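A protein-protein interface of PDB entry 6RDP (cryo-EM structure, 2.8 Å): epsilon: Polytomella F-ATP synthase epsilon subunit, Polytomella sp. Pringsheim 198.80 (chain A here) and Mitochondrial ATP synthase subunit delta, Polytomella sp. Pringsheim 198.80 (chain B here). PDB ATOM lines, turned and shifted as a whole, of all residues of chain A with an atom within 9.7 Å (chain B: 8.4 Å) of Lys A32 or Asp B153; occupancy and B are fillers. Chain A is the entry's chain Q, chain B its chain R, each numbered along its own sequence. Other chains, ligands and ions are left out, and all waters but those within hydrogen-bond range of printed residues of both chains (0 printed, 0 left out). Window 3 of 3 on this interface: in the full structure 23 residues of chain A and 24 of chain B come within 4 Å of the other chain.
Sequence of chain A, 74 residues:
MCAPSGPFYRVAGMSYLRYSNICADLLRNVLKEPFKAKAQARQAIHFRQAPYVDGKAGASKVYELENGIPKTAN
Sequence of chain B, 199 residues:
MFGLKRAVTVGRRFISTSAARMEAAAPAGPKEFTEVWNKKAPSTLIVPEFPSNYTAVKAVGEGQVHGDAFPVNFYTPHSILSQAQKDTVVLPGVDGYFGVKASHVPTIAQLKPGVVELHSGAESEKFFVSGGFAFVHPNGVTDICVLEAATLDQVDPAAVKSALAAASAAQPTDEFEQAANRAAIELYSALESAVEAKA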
ATOM      1  N   LEU A  27     -18.216   0.555 -32.089  1.00  0.00           N
ATOM      2  CA  LEU A  27     -19.367   0.387 -31.210  1.00  0.00           C
ATOM      3  C   LEU A  27     -18.909   0.068 -29.798  1.00  0.00           C
ATOM      4  O   LEU A  27     -19.582   0.422 -28.826  1.00  0.00           O
ATOM      5  CB  LEU A  27     -20.286  -0.720 -31.722  1.00  0.00           C
ATOM      6  CG  LEU A  27     -21.748  -0.804 -31.242  1.00  0.00           C
ATOM      7  CD1 LEU A  27     -22.517  -1.539 -32.297  1.00  0.00           C
ATOM      8  CD2 LEU A  27     -21.996  -1.481 -29.905  1.00  0.00           C
ATOM      9  N   ARG A  28     -17.774  -0.620 -29.667  1.00  0.00           N
ATOM     10  CA  ARG A  28     -17.288  -0.994 -28.345  1.00  0.00           C
ATOM     11  C   ARG A  28     -16.763   0.206 -27.575  1.00  0.00           C
ATOM     12  O   ARG A  28     -16.963   0.292 -26.358  1.00  0.00           O
ATOM     13  CB  ARG A  28     -16.201  -2.061 -28.474  1.00  0.00           C
ATOM     14  CG  ARG A  28     -16.736  -3.477 -28.578  1.00  0.00           C
ATOM     15  CD  ARG A  28     -15.617  -4.493 -28.704  1.00  0.00           C
ATOM     16  NE  ARG A  28     -16.079  -5.752 -29.264  1.00  0.00           N
ATOM     17  CZ  ARG A  28     -15.607  -6.286 -30.381  1.00  0.00           C
ATOM     18  NH1 ARG A  28     -14.640  -5.676 -31.054  1.00  0.00           N
ATOM     19  NH2 ARG A  28     -16.094  -7.436 -30.818  1.00  0.00           N
ATOM     20  N   ASN A  29     -16.119   1.151 -28.267  1.00  0.00           N
ATOM     21  CA  ASN A  29     -15.491   2.297 -27.617  1.00  0.00           C
ATOM     22  C   ASN A  29     -16.478   3.273 -26.981  1.00  0.00           C
ATOM     23  O   ASN A  29     -16.041   4.167 -26.250  1.00  0.00           O
ATOM     24  CB  ASN A  29     -14.636   3.067 -28.619  1.00  0.00           C
ATOM     25  CG  ASN A  29     -13.338   2.377 -28.924  1.00  0.00           C
ATOM     26  OD1 ASN A  29     -13.185   1.186 -28.670  1.00  0.00           O
ATOM     27  ND2 ASN A  29     -12.389   3.121 -29.474  1.00  0.00           N
ATOM     28  N   VAL A  30     -17.776   3.142 -27.240  1.00  0.00           N
ATOM     29  CA  VAL A  30     -18.763   4.101 -26.758  1.00  0.00           C
ATOM     30  C   VAL A  30     -19.761   3.417 -25.834  1.00  0.00           C
ATOM     31  O   VAL A  30     -20.857   3.933 -25.588  1.00  0.00           O
ATOM     32  CB  VAL A  30     -19.474   4.785 -27.938  1.00  0.00           C
ATOM     33  CG1 VAL A  30     -18.476   5.531 -28.799  1.00  0.00           C
ATOM     34  CG2 VAL A  30     -20.178   3.750 -28.785  1.00  0.00           C
ATOM     35  N   LEU A  31     -19.376   2.277 -25.282  1.00  0.00           N
ATOM     36  CA  LEU A  31     -20.282   1.458 -24.495  1.00  0.00           C
ATOM     37  C   LEU A  31     -20.353   1.987 -23.054  1.00  0.00           C
ATOM     38  O   LEU A  31     -19.655   2.932 -22.679  1.00  0.00           O
ATOM     39  CB  LEU A  31     -19.813   0.001 -24.554  1.00  0.00           C
ATOM     40  CG  LEU A  31     -20.731  -1.209 -24.344  1.00  0.00           C
ATOM     41  CD1 LEU A  31     -21.758  -1.302 -25.451  1.00  0.00           C
ATOM     42  CD2 LEU A  31     -19.908  -2.475 -24.312  1.00  0.00           C
ATOM     43  N   LYS A  32     -21.228   1.379 -22.252  1.00  0.00           N
ATOM     44  CA  LYS A  32     -21.357   1.725 -20.838  1.00  0.00           C
ATOM     45  C   LYS A  32     -20.145   1.240 -20.055  1.00  0.00           C
ATOM     46  O   LYS A  32     -19.566   0.203 -20.365  1.00  0.00           O
ATOM     47  CB  LYS A  32     -22.621   1.095 -20.253  1.00  0.00           C
ATOM     48  CG  LYS A  32     -23.153   1.734 -19.000  1.00  0.00           C
ATOM     49  CD  LYS A  32     -24.042   0.761 -18.238  1.00  0.00           C
ATOM     50  CE  LYS A  32     -25.468   0.773 -18.750  1.00  0.00           C
ATOM     51  NZ  LYS A  32     -26.298  -0.287 -18.121  1.00  0.00           N
ATOM     52  N   GLU A  33     -19.773   1.989 -19.014  1.00  0.00           N
ATOM     53  CA  GLU A  33     -18.595   1.673 -18.200  1.00  0.00           C
ATOM     54  C   GLU A  33     -18.699   0.401 -17.349  1.00  0.00           C
ATOM     55  O   GLU A  33     -17.659  -0.211 -17.079  1.00  0.00           O
ATOM     56  CB  GLU A  33     -18.223   2.864 -17.309  1.00  0.00           C
ATOM     57  CG  GLU A  33     -17.673   4.058 -18.068  1.00  0.00           C
ATOM     58  CD  GLU A  33     -18.757   4.985 -18.575  1.00  0.00           C
ATOM     59  OE1 GLU A  33     -19.939   4.754 -18.249  1.00  0.00           O
ATOM     60  OE2 GLU A  33     -18.426   5.942 -19.303  1.00  0.00           O
ATOM     61  N   PRO A  34     -19.880  -0.045 -16.888  1.00  0.00           N
ATOM     62  CA  PRO A  34     -19.985  -1.449 -16.439  1.00  0.00           C
ATOM     63  C   PRO A  34     -19.816  -2.486 -17.545  1.00  0.00           C
ATOM     64  O   PRO A  34     -19.719  -3.679 -17.229  1.00  0.00           O
ATOM     65  CB  PRO A  34     -21.392  -1.522 -15.845  1.00  0.00           C
ATOM     66  CG  PRO A  34     -21.630  -0.189 -15.331  1.00  0.00           C
ATOM     67  CD  PRO A  34     -20.938   0.765 -16.254  1.00  0.00           C
ATOM     68  N   PHE A  35     -19.790  -2.081 -18.817  1.00  0.00           N
ATOM     69  CA  PHE A  35     -19.690  -2.998 -19.939  1.00  0.00           C
ATOM     70  C   PHE A  35     -18.497  -2.723 -20.846  1.00  0.00           C
ATOM     71  O   PHE A  35     -18.057  -3.641 -21.546  1.00  0.00           O
ATOM     72  CB  PHE A  35     -20.968  -2.934 -20.788  1.00  0.00           C
ATOM     73  CG  PHE A  35     -22.211  -3.401 -20.077  1.00  0.00           C
ATOM     74  CD1 PHE A  35     -22.698  -4.680 -20.284  1.00  0.00           C
ATOM     75  CD2 PHE A  35     -22.915  -2.552 -19.238  1.00  0.00           C
ATOM     76  CE1 PHE A  35     -23.846  -5.109 -19.649  1.00  0.00           C
ATOM     77  CE2 PHE A  35     -24.058  -2.976 -18.600  1.00  0.00           C
ATOM     78  CZ  PHE A  35     -24.525  -4.255 -18.805  1.00  0.00           C
ATOM     79  N   LYS A  36     -17.960  -1.500 -20.848  1.00  0.00           N
ATOM     80  CA  LYS A  36     -16.898  -1.153 -21.790  1.00  0.00           C
ATOM     81  C   LYS A  36     -15.578  -1.810 -21.411  1.00  0.00           C
ATOM     82  O   LYS A  36     -14.780  -2.164 -22.288  1.00  0.00           O
ATOM     83  CB  LYS A  36     -16.734   0.364 -21.867  1.00  0.00           C
ATOM     84  CG  LYS A  36     -15.905   0.841 -23.041  1.00  0.00           C
ATOM     85  CD  LYS A  36     -15.373   2.237 -22.811  1.00  0.00           C
ATOM     86  CE  LYS A  36     -14.339   2.583 -23.855  1.00  0.00           C
ATOM     87  NZ  LYS A  36     -13.363   1.476 -24.012  1.00  0.00           N
ATOM     88  N   ALA A  37     -15.327  -1.971 -20.111  1.00  0.00           N
ATOM     89  CA  ALA A  37     -14.081  -2.592 -19.671  1.00  0.00           C
ATOM     90  C   ALA A  37     -14.075  -4.086 -19.962  1.00  0.00           C
ATOM     91  O   ALA A  37     -13.046  -4.639 -20.362  1.00  0.00           O
ATOM     92  CB  ALA A  37     -13.859  -2.331 -18.182  1.00  0.00           C
ATOM     93  N   LYS A  38     -15.214  -4.755 -19.777  1.00  0.00           N
ATOM     94  CA  LYS A  38     -15.296  -6.170 -20.114  1.00  0.00           C
ATOM     95  C   LYS A  38     -15.470  -6.400 -21.606  1.00  0.00           C
ATOM     96  O   LYS A  38     -15.293  -7.529 -22.070  1.00  0.00           O
ATOM     97  CB  LYS A  38     -16.440  -6.842 -19.351  1.00  0.00           C
ATOM     98  CG  LYS A  38     -17.823  -6.343 -19.719  1.00  0.00           C
ATOM     99  CD  LYS A  38     -18.905  -7.206 -19.107  1.00  0.00           C
ATOM    100  CE  LYS A  38     -18.764  -8.649 -19.554  1.00  0.00           C
ATOM    101  NZ  LYS A  38     -18.681  -8.766 -21.037  1.00  0.00           N
ATOM    102  N   ALA A  39     -15.823  -5.363 -22.365  1.00  0.00           N
ATOM    103  CA  ALA A  39     -15.758  -5.448 -23.816  1.00  0.00           C
ATOM    104  C   ALA A  39     -14.360  -5.185 -24.353  1.00  0.00           C
ATOM    105  O   ALA A  39     -14.153  -5.260 -25.566  1.00  0.00           O
ATOM    106  CB  ALA A  39     -16.742  -4.465 -24.445  1.00  0.00           C
ATOM    107  N   GLN A  40     -13.406  -4.853 -23.487  1.00  0.00           N
ATOM    108  CA  GLN A  40     -12.020  -4.763 -23.911  1.00  0.00           C
ATOM    109  C   GLN A  40     -11.347  -6.127 -23.904  1.00  0.00           C
ATOM    110  O   GLN A  40     -10.289  -6.292 -24.524  1.00  0.00           O
ATOM    111  CB  GLN A  40     -11.267  -3.784 -23.009  1.00  0.00           C
ATOM    112  CG  GLN A  40     -10.061  -3.130 -23.644  1.00  0.00           C
ATOM    113  CD  GLN A  40     -10.389  -2.422 -24.933  1.00  0.00           C
ATOM    114  OE1 GLN A  40     -10.011  -2.877 -26.015  1.00  0.00           O
ATOM    115  NE2 GLN A  40     -11.093  -1.300 -24.829  1.00  0.00           N
ATOM    116  N   ARG A  42     -12.735  -8.885 -25.234  1.00  0.00           N
ATOM    117  CA  ARG A  42     -13.033  -9.413 -26.557  1.00  0.00           C
ATOM    118  C   ARG A  42     -12.481  -8.547 -27.678  1.00  0.00           C
ATOM    119  O   ARG A  42     -12.887  -8.716 -28.829  1.00  0.00           O
ATOM    120  CB  ARG A  42     -14.540  -9.560 -26.725  1.00  0.00           C
ATOM    121  CG  ARG A  42     -15.275  -8.271 -26.496  1.00  0.00           C
ATOM    122  CD  ARG A  42     -16.711  -8.394 -26.903  1.00  0.00           C
ATOM    123  NE  ARG A  42     -17.444  -9.301 -26.032  1.00  0.00           N
ATOM    124  CZ  ARG A  42     -18.348  -8.906 -25.146  1.00  0.00           C
ATOM    125  NH1 ARG A  42     -18.974  -9.795 -24.391  1.00  0.00           N
ATOM    126  NH2 ARG A  42     -18.631  -7.619 -25.016  1.00  0.00           N
ATOM    127  N   SER B 124     -40.549  -5.486 -26.278  1.00  0.00           N
ATOM    128  CA  SER B 124     -39.534  -5.360 -27.312  1.00  0.00           C
ATOM    129  C   SER B 124     -38.172  -5.203 -26.659  1.00  0.00           C
ATOM    130  O   SER B 124     -37.996  -4.337 -25.798  1.00  0.00           O
ATOM    131  CB  SER B 124     -39.824  -4.152 -28.213  1.00  0.00           C
ATOM    132  OG  SER B 124     -38.668  -3.743 -28.922  1.00  0.00           O
ATOM    133  N   GLU B 125     -37.217  -6.033 -27.067  1.00  0.00           N
ATOM    134  CA  GLU B 125     -35.829  -5.870 -26.656  1.00  0.00           C
ATOM    135  C   GLU B 125     -35.023  -5.346 -27.838  1.00  0.00           C
ATOM    136  O   GLU B 125     -35.051  -5.921 -28.931  1.00  0.00           O
ATOM    137  CB  GLU B 125     -35.242  -7.176 -26.110  1.00  0.00           C
ATOM    138  CG  GLU B 125     -35.420  -8.414 -26.963  1.00  0.00           C
ATOM    139  CD  GLU B 125     -36.642  -9.228 -26.614  1.00  0.00           C
ATOM    140  OE1 GLU B 125     -37.636  -8.644 -26.139  1.00  0.00           O
ATOM    141  OE2 GLU B 125     -36.606 -10.457 -26.826  1.00  0.00           O
ATOM    142  N   LYS B 126     -34.328  -4.238 -27.618  1.00  0.00           N
ATOM    143  CA  LYS B 126     -33.689  -3.475 -28.681  1.00  0.00           C
ATOM    144  C   LYS B 126     -32.186  -3.665 -28.580  1.00  0.00           C
ATOM    145  O   LYS B 126     -31.541  -3.099 -27.694  1.00  0.00           O
ATOM    146  CB  LYS B 126     -34.064  -1.998 -28.583  1.00  0.00           C
ATOM    147  CG  LYS B 126     -35.519  -1.705 -28.924  1.00  0.00           C
ATOM    148  CD  LYS B 126     -35.861  -0.245 -28.672  1.00  0.00           C
ATOM    149  CE  LYS B 126     -35.145   0.667 -29.655  1.00  0.00           C
ATOM    150  NZ  LYS B 126     -35.528   2.090 -29.483  1.00  0.00           N
ATOM    151  N   PHE B 127     -31.634  -4.465 -29.487  1.00  0.00           N
ATOM    152  CA  PHE B 127     -30.198  -4.646 -29.615  1.00  0.00           C
ATOM    153  C   PHE B 127     -29.704  -3.761 -30.747  1.00  0.00           C
ATOM    154  O   PHE B 127     -30.165  -3.895 -31.882  1.00  0.00           O
ATOM    155  CB  PHE B 127     -29.844  -6.102 -29.911  1.00  0.00           C
ATOM    156  CG  PHE B 127     -30.332  -7.072 -28.887  1.00  0.00           C
ATOM    157  CD1 PHE B 127     -29.600  -7.314 -27.744  1.00  0.00           C
ATOM    158  CD2 PHE B 127     -31.522  -7.758 -29.079  1.00  0.00           C
ATOM    159  CE1 PHE B 127     -30.047  -8.221 -26.807  1.00  0.00           C
ATOM    160  CE2 PHE B 127     -31.970  -8.667 -28.149  1.00  0.00           C
ATOM    161  CZ  PHE B 127     -31.239  -8.895 -27.012  1.00  0.00           C
ATOM    162  N   PHE B 128     -28.780  -2.860 -30.444  1.00  0.00           N
ATOM    163  CA  PHE B 128     -28.083  -2.118 -31.481  1.00  0.00           C
ATOM    164  C   PHE B 128     -26.844  -2.898 -31.884  1.00  0.00           C
ATOM    165  O   PHE B 128     -25.958  -3.132 -31.056  1.00  0.00           O
ATOM    166  CB  PHE B 128     -27.695  -0.721 -31.017  1.00  0.00           C
ATOM    167  CG  PHE B 128     -26.980   0.077 -32.063  1.00  0.00           C
ATOM    168  CD1 PHE B 128     -27.672   0.607 -33.136  1.00  0.00           C
ATOM    169  CD2 PHE B 128     -25.623   0.303 -31.973  1.00  0.00           C
ATOM    170  CE1 PHE B 128     -27.020   1.342 -34.103  1.00  0.00           C
ATOM    171  CE2 PHE B 128     -24.966   1.037 -32.939  1.00  0.00           C
ATOM    172  CZ  PHE B 128     -25.668   1.557 -34.004  1.00  0.00           C
ATOM    173  N   ALA B 150     -24.759  -5.069 -29.095  1.00  0.00           N
ATOM    174  CA  ALA B 150     -25.030  -4.544 -27.769  1.00  0.00           C
ATOM    175  C   ALA B 150     -26.509  -4.247 -27.604  1.00  0.00           C
ATOM    176  O   ALA B 150     -27.184  -3.847 -28.552  1.00  0.00           O
ATOM    177  CB  ALA B 150     -24.222  -3.271 -27.522  1.00  0.00           C
ATOM    178  N   THR B 151     -27.011  -4.460 -26.395  1.00  0.00           N
ATOM    179  CA  THR B 151     -28.273  -3.856 -26.008  1.00  0.00           C
ATOM    180  C   THR B 151     -28.080  -2.339 -25.972  1.00  0.00           C
ATOM    181  O   THR B 151     -27.020  -1.841 -25.594  1.00  0.00           O
ATOM    182  CB  THR B 151     -28.724  -4.426 -24.652  1.00  0.00           C
ATOM    183  OG1 THR B 151     -29.102  -5.796 -24.823  1.00  0.00           O
ATOM    184  CG2 THR B 151     -29.916  -3.688 -24.068  1.00  0.00           C
ATOM    185  N   LEU B 152     -29.095  -1.600 -26.423  1.00  0.00           N
ATOM    186  CA  LEU B 152     -29.003  -0.145 -26.500  1.00  0.00           C
ATOM    187  C   LEU B 152     -29.054   0.524 -25.123  1.00  0.00           C
ATOM    188  O   LEU B 152     -28.847   1.740 -25.027  1.00  0.00           O
ATOM    189  CB  LEU B 152     -30.114   0.362 -27.428  1.00  0.00           C
ATOM    190  CG  LEU B 152     -30.216   1.794 -27.948  1.00  0.00           C
ATOM    191  CD1 LEU B 152     -29.061   2.098 -28.871  1.00  0.00           C
ATOM    192  CD2 LEU B 152     -31.517   1.952 -28.696  1.00  0.00           C
ATOM    193  N   ASP B 153     -29.301  -0.245 -24.057  1.00  0.00           N
ATOM    194  CA  ASP B 153     -29.180   0.273 -22.700  1.00  0.00           C
ATOM    195  C   ASP B 153     -27.748   0.669 -22.372  1.00  0.00           C
ATOM    196  O   ASP B 153     -27.526   1.682 -21.701  1.00  0.00           O
ATOM    197  CB  ASP B 153     -29.655  -0.777 -21.696  1.00  0.00           C
ATOM    198  CG  ASP B 153     -31.154  -0.762 -21.498  1.00  0.00           C
ATOM    199  OD1 ASP B 153     -31.791   0.270 -21.792  1.00  0.00           O
ATOM    200  OD2 ASP B 153     -31.696  -1.792 -21.046  1.00  0.00           O
ATOM    201  N   GLN B 154     -26.767  -0.097 -22.844  1.00  0.00           N
ATOM    202  CA  GLN B 154     -25.396   0.043 -22.376  1.00  0.00           C
ATOM    203  C   GLN B 154     -24.527   0.887 -23.306  1.00  0.00           C
ATOM    204  O   GLN B 154     -23.322   0.669 -23.399  1.00  0.00           O
ATOM    205  CB  GLN B 154     -24.766  -1.331 -22.140  1.00  0.00           C
ATOM    206  CG  GLN B 154     -24.781  -2.270 -23.323  1.00  0.00           C
ATOM    207  CD  GLN B 154     -25.083  -3.704 -22.928  1.00  0.00           C
ATOM    208  OE1 GLN B 154     -26.079  -3.979 -22.261  1.00  0.00           O
ATOM    209  NE2 GLN B 154     -24.228  -4.627 -23.351  1.00  0.00           N
ATOM    210  N   VAL B 155     -25.109   1.877 -23.972  1.00  0.00           N
ATOM    211  CA  VAL B 155     -24.337   2.857 -24.724  1.00  0.00           C
ATOM    212  C   VAL B 155     -24.578   4.230 -24.104  1.00  0.00           C
ATOM    213  O   VAL B 155     -25.692   4.536 -23.665  1.00  0.00           O
ATOM    214  CB  VAL B 155     -24.691   2.821 -26.231  1.00  0.00           C
ATOM    215  CG1 VAL B 155     -26.172   3.089 -26.483  1.00  0.00           C
ATOM    216  CG2 VAL B 155     -23.818   3.770 -27.034  1.00  0.00           C
ATOM    217  N   ASP B 156     -23.435   5.094 -23.996  1.00  0.00           N
ATOM    218  CA  ASP B 156     -23.873   6.376 -23.460  1.00  0.00           C
ATOM    219  C   ASP B 156     -24.167   7.373 -24.581  1.00  0.00           C
ATOM    220  O   ASP B 156     -23.556   7.316 -25.652  1.00  0.00           O
ATOM    221  CB  ASP B 156     -22.841   6.951 -22.473  1.00  0.00           C
ATOM    222  CG  ASP B 156     -21.420   7.046 -23.033  1.00  0.00           C
ATOM    223  OD1 ASP B 156     -20.503   7.264 -22.212  1.00  0.00           O
ATOM    224  OD2 ASP B 156     -21.185   6.882 -24.244  1.00  0.00           O
ATOM    225  N   PRO B 157     -25.126   8.280 -24.383  1.00  0.00           N
ATOM    226  CA  PRO B 157     -25.422   9.283 -25.413  1.00  0.00           C
ATOM    227  C   PRO B 157     -24.410  10.413 -25.510  1.00  0.00           C
ATOM    228  O   PRO B 157     -24.566  11.277 -26.379  1.00  0.00           O
ATOM    229  CB  PRO B 157     -26.793   9.818 -24.979  1.00  0.00           C
ATOM    230  CG  PRO B 157     -26.861   9.548 -23.519  1.00  0.00           C
ATOM    231  CD  PRO B 157     -26.155   8.255 -23.328  1.00  0.00           C
ATOM    232  N   ALA B 159     -20.669  10.105 -25.573  1.00  0.00           N
ATOM    233  CA  ALA B 159     -19.447   9.828 -26.317  1.00  0.00           C
ATOM    234  C   ALA B 159     -19.660   9.712 -27.819  1.00  0.00           C
ATOM    235  O   ALA B 159     -18.674   9.724 -28.562  1.00  0.00           O
ATOM    236  CB  ALA B 159     -18.801   8.539 -25.804  1.00  0.00           C
ATOM    237  N   VAL B 195     -30.424   6.710 -30.552  1.00  0.00           N
ATOM    238  CA  VAL B 195     -30.470   7.034 -29.129  1.00  0.00           C
ATOM    239  C   VAL B 195     -31.345   8.252 -28.826  1.00  0.00           C
ATOM    240  O   VAL B 195     -31.920   8.318 -27.726  1.00  0.00           O
ATOM    241  CB  VAL B 195     -29.044   7.203 -28.539  1.00  0.00           C
ATOM    242  CG1 VAL B 195     -28.385   8.528 -28.927  1.00  0.00           C
ATOM    243  CG2 VAL B 195     -29.030   6.997 -27.021  1.00  0.00           C
ATOM    244  N   LYS B 198     -35.702   7.109 -28.754  1.00  0.00           N
ATOM    245  CA  LYS B 198     -36.189   6.050 -27.888  1.00  0.00           C
ATOM    246  C   LYS B 198     -37.708   6.111 -27.745  1.00  0.00           C
ATOM    247  O   LYS B 198     -38.340   7.155 -27.934  1.00  0.00           O
ATOM    248  CB  LYS B 198     -35.534   6.138 -26.512  1.00  0.00           C
ATOM    249  CG  LYS B 198     -34.027   6.022 -26.551  1.00  0.00           C
ATOM    250  CD  LYS B 198     -33.497   5.322 -25.313  1.00  0.00           C
ATOM    251  CE  LYS B 198     -32.001   5.121 -25.413  1.00  0.00           C
ATOM    252  NZ  LYS B 198     -31.619   4.749 -26.795  1.00  0.00           N
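The backbone carbonyl oxygen of Val A30 sits at hydrogen-bond distance from the backbone NH of Asp B156. The backbone NH (N) of Lys A32 sits at hydrogen-bond distance from the backbone carbonyl oxygen (O) of Gln B154, 2.5 Å away.
Printed residues of chain A that touch a printed residue of chain B: Leu A27, Val A30, Leu A31, Lys A32, Glu A33 and Phe A35. Of the 16 printed residues of chain B, 6 touch a printed residue of chain A. Among the printed residues, 10 pairs touch across the chains.
Among the printed residues, merely in contact across the chains: Leu A31 with Gln B154 (3.2 Å), Val A30 with Val B155 (3.3 Å), Phe A35 with Gln B154 (3.4 Å), Leu A27 with Phe B128 (3.6 Å), Lys A32 with Asp B153 (3.7 Å), Leu A27 with Ala B150 (3.7 Å), Leu A31 with Ala B150 (3.8 Å) and Glu A33 with Asp B156 (3.8 Å).
The backbone carbonyl oxygen of Ala B150 lies within hydrogen-bond range of the backbone NH of Phe B128 (2.7 Å).
Lys A32 touches just these residues of chain B: Asp B153 (3.7 Å) and Gln B154 (2.5 Å). Asp B153 touches just one residue of chain A: Lys A32. No residue of chain A comes within 4 Å of Thr B151. No residue of chain A comes within 4 Å of Leu B152. Of the printed residues of chain A, Ala B150 touches Leu A27 (3.7 Å) and Leu A31 (3.8 Å). Of the printed residues of chain B, Phe A35 touches Gln B154 (3.4 Å). Printed residues of chain B within 4 Å of Val A30: Val B155 (3.3 Å) and Asp B156 (3.2 Å). Printed residues of chain A within 4 Å of Phe B128: Leu A27. Printed residues of chain B within 4 Å of Leu A31: Ala B150 and Gln B154. The nearest residue of chain A that does not touch Asp B153 is Phe A35 (6.4 Å). The nearest printed residue of chain B that does not touch Glu A33 is Gln B154 (5.8 Å).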
